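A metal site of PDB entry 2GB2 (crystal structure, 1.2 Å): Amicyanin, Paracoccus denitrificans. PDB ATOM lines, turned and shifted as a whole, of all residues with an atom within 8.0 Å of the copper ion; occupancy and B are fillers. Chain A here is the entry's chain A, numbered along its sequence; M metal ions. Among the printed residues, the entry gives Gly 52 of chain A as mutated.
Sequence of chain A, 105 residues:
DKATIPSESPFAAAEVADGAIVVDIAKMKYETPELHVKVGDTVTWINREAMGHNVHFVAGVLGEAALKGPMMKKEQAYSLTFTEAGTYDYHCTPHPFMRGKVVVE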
ATOM      1  N   ILE A  25       7.215  16.788 -33.725  1.00  0.00           N
ATOM      2  CA  ILE A  25       7.704  16.505 -32.374  1.00  0.00           C
ATOM      3  C   ILE A  25       8.360  15.143 -32.425  1.00  0.00           C
ATOM      4  O   ILE A  25       7.707  14.155 -32.708  1.00  0.00           O
ATOM      5  CB  ILE A  25       6.575  16.591 -31.334  1.00  0.00           C
ATOM      6  CG1 ILE A  25       5.686  17.838 -31.434  1.00  0.00           C
ATOM      7  CG2 ILE A  25       7.166  16.519 -29.946  1.00  0.00           C
ATOM      8  CD1 ILE A  25       4.444  17.793 -30.535  1.00  0.00           C
ATOM      9  N   MET A  28      11.912  13.912 -28.221  1.00  0.00           N
ATOM     10  CA  MET A  28      11.591  14.698 -27.057  1.00  0.00           C
ATOM     11  C   MET A  28      11.880  16.200 -27.243  1.00  0.00           C
ATOM     12  O   MET A  28      12.271  16.882 -26.301  1.00  0.00           O
ATOM     13  CB  MET A  28      12.307  14.190 -25.815  1.00  0.00           C
ATOM     14  CG  MET A  28      11.884  12.791 -25.454  1.00  0.00           C
ATOM     15  SD  MET A  28      10.185  12.544 -24.901  1.00  0.00           S
ATOM     16  CE  MET A  28      10.098  13.673 -23.504  1.00  0.00           C
ATOM     17  N   LYS A  29      11.688  16.682 -28.447  1.00  0.00           N
ATOM     18  CA  LYS A  29      11.916  18.079 -28.806  1.00  0.00           C
ATOM     19  C   LYS A  29      10.876  18.511 -29.819  1.00  0.00           C
ATOM     20  O   LYS A  29      10.473  17.722 -30.692  1.00  0.00           O
ATOM     21  CB  LYS A  29      13.318  18.258 -29.433  1.00  0.00           C
ATOM     22  CG  LYS A  29      14.471  17.798 -28.559  1.00  0.00           C
ATOM     23  CD  LYS A  29      15.756  17.922 -29.357  1.00  0.00           C
ATOM     24  CE  LYS A  29      16.425  16.576 -29.551  1.00  0.00           C
ATOM     25  NZ  LYS A  29      17.871  16.704 -29.881  1.00  0.00           N
ATOM     26  N   TYR A  30      10.558  19.800 -29.784  1.00  0.00           N
ATOM     27  CA  TYR A  30       9.909  20.411 -30.941  1.00  0.00           C
ATOM     28  C   TYR A  30      10.962  20.626 -32.029  1.00  0.00           C
ATOM     29  O   TYR A  30      11.953  21.335 -31.798  1.00  0.00           O
ATOM     30  CB  TYR A  30       9.244  21.728 -30.558  1.00  0.00           C
ATOM     31  CG  TYR A  30       8.247  21.659 -29.435  1.00  0.00           C
ATOM     32  CD1 TYR A  30       7.016  21.010 -29.644  1.00  0.00           C
ATOM     33  CD2 TYR A  30       8.414  22.219 -28.178  1.00  0.00           C
ATOM     34  CE1 TYR A  30       6.075  20.912 -28.652  1.00  0.00           C
ATOM     35  CE2 TYR A  30       7.469  22.150 -27.199  1.00  0.00           C
ATOM     36  CZ  TYR A  30       6.294  21.499 -27.428  1.00  0.00           C
ATOM     37  OH  TYR A  30       5.343  21.460 -26.412  1.00  0.00           O
ATOM     38  N   ASN A  47       2.914  14.794 -33.520  1.00  0.00           N
ATOM     39  CA  ASN A  47       3.746  13.953 -32.656  1.00  0.00           C
ATOM     40  C   ASN A  47       4.206  12.727 -33.442  1.00  0.00           C
ATOM     41  O   ASN A  47       3.377  11.954 -33.933  1.00  0.00           O
ATOM     42  CB  ASN A  47       2.951  13.571 -31.415  1.00  0.00           C
ATOM     43  CG  ASN A  47       3.814  12.842 -30.405  1.00  0.00           C
ATOM     44  OD1 ASN A  47       5.036  12.780 -30.623  1.00  0.00           O
ATOM     45  ND2 ASN A  47       3.206  12.329 -29.340  1.00  0.00           N
ATOM     46  N   GLU A  49       6.412  10.570 -32.119  1.00  0.00           N
ATOM     47  CA  GLU A  49       6.971   9.630 -31.136  1.00  0.00           C
ATOM     48  C   GLU A  49       5.928   8.864 -30.315  1.00  0.00           C
ATOM     49  O   GLU A  49       4.830   9.413 -30.246  1.00  0.00           O
ATOM     50  CB  GLU A  49       7.711  10.321 -29.989  1.00  0.00           C
ATOM     51  CG  GLU A  49       8.813  11.286 -30.322  1.00  0.00           C
ATOM     52  CD  GLU A  49       9.659  11.484 -29.088  1.00  0.00           C
ATOM     53  OE1 GLU A  49       9.348  12.389 -28.294  1.00  0.00           O
ATOM     54  OE2 GLU A  49      10.641  10.782 -28.862  1.00  0.00           O
ATOM     55  N   MET A  51       5.867   8.616 -26.983  1.00  0.00           N
ATOM     56  CA  MET A  51       5.475   9.404 -25.811  1.00  0.00           C
ATOM     57  C   MET A  51       4.522  10.532 -26.192  1.00  0.00           C
ATOM     58  O   MET A  51       4.779  11.237 -27.184  1.00  0.00           O
ATOM     59  CB  MET A  51       6.730   9.985 -25.168  1.00  0.00           C
ATOM     60  CG  MET A  51       6.441  10.662 -23.831  1.00  0.00           C
ATOM     61  SD  MET A  51       5.189   9.816 -22.859  1.00  0.00           S
ATOM     62  CE  MET A  51       6.201   8.677 -21.915  1.00  0.00           C
ATOM     63  N   GLY A  52       3.459  10.729 -25.432  1.00  0.00           N
ATOM     64  CA  GLY A  52       2.525  11.829 -25.611  1.00  0.00           C
ATOM     65  C   GLY A  52       3.133  13.191 -25.309  1.00  0.00           C
ATOM     66  O   GLY A  52       3.903  13.381 -24.377  1.00  0.00           O
ATOM     67  N   HIS A  53       2.720  14.171 -26.077  1.00  0.00           N
ATOM     68  CA  HIS A  53       3.162  15.546 -25.998  1.00  0.00           C
ATOM     69  C   HIS A  53       1.992  16.497 -26.293  1.00  0.00           C
ATOM     70  O   HIS A  53       1.070  16.107 -27.024  1.00  0.00           O
ATOM     71  CB  HIS A  53       4.269  15.870 -26.986  1.00  0.00           C
ATOM     72  CG  HIS A  53       5.490  15.042 -26.841  1.00  0.00           C
ATOM     73  ND1 HIS A  53       6.363  15.178 -25.765  1.00  0.00           N
ATOM     74  CD2 HIS A  53       6.008  14.086 -27.634  1.00  0.00           C
ATOM     75  CE1 HIS A  53       7.338  14.360 -25.906  1.00  0.00           C
ATOM     76  NE2 HIS A  53       7.176  13.674 -27.034  1.00  0.00           N
ATOM     77  N   ASN A  54       2.086  17.725 -25.776  1.00  0.00           N
ATOM     78  CA  ASN A  54       1.101  18.732 -26.207  1.00  0.00           C
ATOM     79  C   ASN A  54       1.856  20.045 -26.465  1.00  0.00           C
ATOM     80  O   ASN A  54       3.108  20.049 -26.468  1.00  0.00           O
ATOM     81  CB  ASN A  54      -0.014  18.873 -25.188  1.00  0.00           C
ATOM     82  CG  ASN A  54       0.402  19.608 -23.962  1.00  0.00           C
ATOM     83  OD1 ASN A  54       1.578  19.696 -23.654  1.00  0.00           O
ATOM     84  ND2 ASN A  54      -0.618  20.124 -23.320  1.00  0.00           N
ATOM     85  N   VAL A  55       1.120  21.097 -26.679  1.00  0.00           N
ATOM     86  CA  VAL A  55       1.583  22.456 -26.657  1.00  0.00           C
ATOM     87  C   VAL A  55       0.780  23.263 -25.616  1.00  0.00           C
ATOM     88  O   VAL A  55      -0.442  23.087 -25.528  1.00  0.00           O
ATOM     89  CB  VAL A  55       1.597  23.148 -28.033  1.00  0.00           C
ATOM     90  CG1 VAL A  55       2.531  22.396 -28.985  1.00  0.00           C
ATOM     91  CG2 VAL A  55       0.194  23.230 -28.643  1.00  0.00           C
ATOM     92  N   MET A  71      -3.314  16.327 -25.345  1.00  0.00           N
ATOM     93  CA  MET A  71      -2.224  15.377 -25.493  1.00  0.00           C
ATOM     94  C   MET A  71      -2.366  14.658 -26.835  1.00  0.00           C
ATOM     95  O   MET A  71      -3.453  14.131 -27.102  1.00  0.00           O
ATOM     96  CB  MET A  71      -2.195  14.401 -24.330  1.00  0.00           C
ATOM     97  CG  MET A  71      -1.907  15.088 -22.991  1.00  0.00           C
ATOM     98  SD  MET A  71      -0.253  15.841 -22.913  1.00  0.00           S
ATOM     99  CE  MET A  71       0.722  14.383 -23.178  1.00  0.00           C
ATOM    100  N   MET A  72      -1.304  14.693 -27.624  1.00  0.00           N
ATOM    101  CA  MET A  72      -1.223  14.037 -28.911  1.00  0.00           C
ATOM    102  C   MET A  72      -0.579  12.673 -28.756  1.00  0.00           C
ATOM    103  O   MET A  72       0.537  12.635 -28.225  1.00  0.00           O
ATOM    104  CB  MET A  72      -0.384  14.839 -29.927  1.00  0.00           C
ATOM    105  CG  MET A  72      -1.089  16.056 -30.524  1.00  0.00           C
ATOM    106  SD  MET A  72       0.039  17.156 -31.420  1.00  0.00           S
ATOM    107  CE  MET A  72       0.692  18.057 -30.003  1.00  0.00           C
ATOM    108  N   HIS A  91       5.311  25.477 -24.163  1.00  0.00           N
ATOM    109  CA  HIS A  91       6.047  24.317 -23.656  1.00  0.00           C
ATOM    110  C   HIS A  91       5.137  23.111 -23.657  1.00  0.00           C
ATOM    111  O   HIS A  91       3.947  23.179 -23.925  1.00  0.00           O
ATOM    112  CB  HIS A  91       6.572  24.580 -22.252  1.00  0.00           C
ATOM    113  CG  HIS A  91       5.498  24.685 -21.187  1.00  0.00           C
ATOM    114  ND1 HIS A  91       4.827  25.844 -20.995  1.00  0.00           N
ATOM    115  CD2 HIS A  91       4.974  23.779 -20.331  1.00  0.00           C
ATOM    116  CE1 HIS A  91       3.931  25.666 -20.006  1.00  0.00           C
ATOM    117  NE2 HIS A  91       4.016  24.395 -19.579  1.00  0.00           N
ATOM    118  N   CYS A  92       5.679  21.937 -23.372  1.00  0.00           N
ATOM    119  CA  CYS A  92       4.927  20.693 -23.217  1.00  0.00           C
ATOM    120  C   CYS A  92       4.538  20.480 -21.755  1.00  0.00           C
ATOM    121  O   CYS A  92       5.374  20.491 -20.880  1.00  0.00           O
ATOM    122  CB  CYS A  92       5.716  19.550 -23.841  1.00  0.00           C
ATOM    123  SG  CYS A  92       4.846  17.968 -23.650  1.00  0.00           S
ATOM    124  N   THR A  93       3.266  20.331 -21.449  1.00  0.00           N
ATOM    125  CA  THR A  93       2.795  20.277 -20.070  1.00  0.00           C
ATOM    126  C   THR A  93       3.485  19.178 -19.286  1.00  0.00           C
ATOM    127  O   THR A  93       3.991  19.498 -18.228  1.00  0.00           O
ATOM    128  CB  THR A  93       1.256  20.124 -20.037  1.00  0.00           C
ATOM    129  OG1 THR A  93       0.671  21.254 -20.665  1.00  0.00           O
ATOM    130  CG2 THR A  93       0.749  20.037 -18.596  1.00  0.00           C
ATOM    131  N   PRO A  94       3.501  17.901 -19.681  1.00  0.00           N
ATOM    132  CA  PRO A  94       4.166  16.842 -18.918  1.00  0.00           C
ATOM    133  C   PRO A  94       5.684  16.962 -18.970  1.00  0.00           C
ATOM    134  O   PRO A  94       6.350  16.474 -18.032  1.00  0.00           O
ATOM    135  CB  PRO A  94       3.707  15.525 -19.597  1.00  0.00           C
ATOM    136  CG  PRO A  94       3.415  15.977 -20.994  1.00  0.00           C
ATOM    137  CD  PRO A  94       2.767  17.341 -20.842  1.00  0.00           C
ATOM    138  N   HIS A  95       6.233  17.626 -20.002  1.00  0.00           N
ATOM    139  CA  HIS A  95       7.666  17.786 -20.206  1.00  0.00           C
ATOM    140  C   HIS A  95       8.104  19.226 -20.382  1.00  0.00           C
ATOM    141  O   HIS A  95       8.456  19.714 -21.447  1.00  0.00           O
ATOM    142  CB  HIS A  95       8.105  17.021 -21.469  1.00  0.00           C
ATOM    143  CG  HIS A  95       7.566  15.632 -21.489  1.00  0.00           C
ATOM    144  ND1 HIS A  95       6.827  15.175 -22.570  1.00  0.00           N
ATOM    145  CD2 HIS A  95       7.669  14.603 -20.637  1.00  0.00           C
ATOM    146  CE1 HIS A  95       6.465  13.919 -22.357  1.00  0.00           C
ATOM    147  NE2 HIS A  95       6.965  13.529 -21.187  1.00  0.00           N
ATOM    148  N   PRO A  96       8.063  20.013 -19.309  1.00  0.00           N
ATOM    149  CA  PRO A  96       8.299  21.457 -19.505  1.00  0.00           C
ATOM    150  C   PRO A  96       9.699  21.852 -19.967  1.00  0.00           C
ATOM    151  O   PRO A  96       9.892  23.027 -20.319  1.00  0.00           O
ATOM    152  CB  PRO A  96       7.980  22.065 -18.128  1.00  0.00           C
ATOM    153  CG  PRO A  96       8.028  20.920 -17.186  1.00  0.00           C
ATOM    154  CD  PRO A  96       7.647  19.686 -17.951  1.00  0.00           C
ATOM    155  N   PHE A  97      10.645  20.908 -19.954  1.00  0.00           N
ATOM    156  CA  PHE A  97      11.942  21.205 -20.587  1.00  0.00           C
ATOM    157  C   PHE A  97      11.815  21.317 -22.090  1.00  0.00           C
ATOM    158  O   PHE A  97      12.770  21.798 -22.722  1.00  0.00           O
ATOM    159  CB  PHE A  97      12.947  20.103 -20.241  1.00  0.00           C
ATOM    160  CG  PHE A  97      12.430  18.684 -20.462  1.00  0.00           C
ATOM    161  CD1 PHE A  97      12.511  18.050 -21.703  1.00  0.00           C
ATOM    162  CD2 PHE A  97      11.843  17.999 -19.413  1.00  0.00           C
ATOM    163  CE1 PHE A  97      12.069  16.742 -21.847  1.00  0.00           C
ATOM    164  CE2 PHE A  97      11.348  16.713 -19.541  1.00  0.00           C
ATOM    165  CZ  PHE A  97      11.413  16.118 -20.797  1.00  0.00           C
ATOM    166  N   MET A  98      10.717  20.888 -22.697  1.00  0.00           N
ATOM    167  CA  MET A  98      10.426  21.096 -24.114  1.00  0.00           C
ATOM    168  C   MET A  98       9.831  22.495 -24.267  1.00  0.00           C
ATOM    169  O   MET A  98       8.705  22.695 -23.843  1.00  0.00           O
ATOM    170  CB  MET A  98       9.484  20.021 -24.592  1.00  0.00           C
ATOM    171  CG  MET A  98      10.025  18.585 -24.497  1.00  0.00           C
ATOM    172  SD  MET A  98       8.772  17.376 -25.077  1.00  0.00           S
ATOM    173  CE  MET A  98       8.449  17.996 -26.747  1.00  0.00           C
HETATM  174 CU    CU M   1       6.214  16.382 -24.217  1.00  0.00          CU
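The copper ion is bound by a ring nitrogen (ND1) of His 53 (2.0 Å), a ring nitrogen (ND1) of His 95 (2.1 Å) and the side-chain sulfur (SG) of Cys 92 (2.2 Å).
Slightly farther from the copper ion lies SD of Met 98 (2.9 Å).
The side-chain sulfur (SG) of Cys 92 lies close to the backbone NH (N) of Asn 54 (3.5 Å).
The backbone NH (N) of Cys 92 lies within hydrogen-bond range of the side-chain hydroxyl (OH) of Tyr 30, 3.1 Å away.
The side-chain carboxylate (OE1) of Glu 49 is in hydrogen-bond range of a ring nitrogen (NE2) of His 53 (2.8 Å).
The backbone carbonyl oxygen of Met 51 lies close to a ring nitrogen (NE2) of His 53 (3.4 Å).
A ring nitrogen (ND1) of His 53 lies close to the side-chain sulfur (SD) of Met 98, 3.3 Å away.
N of Met 72 is in hydrogen-bond range of O of His 53.
The backbone NH (N) of Cys 92 is in hydrogen-bond range of the backbone carbonyl oxygen (O) of Met 98, 3.2 Å away.
Merely in contact with the copper ion: Gly 52 (3.8 Å).
Five residues have an atom within 4 Å of the copper ion: Gly 52, His 53, Cys 92, His 95 and Met 98.
The nearest printed residue that does not touch the copper ion is Pro 94 (4.3 Å).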
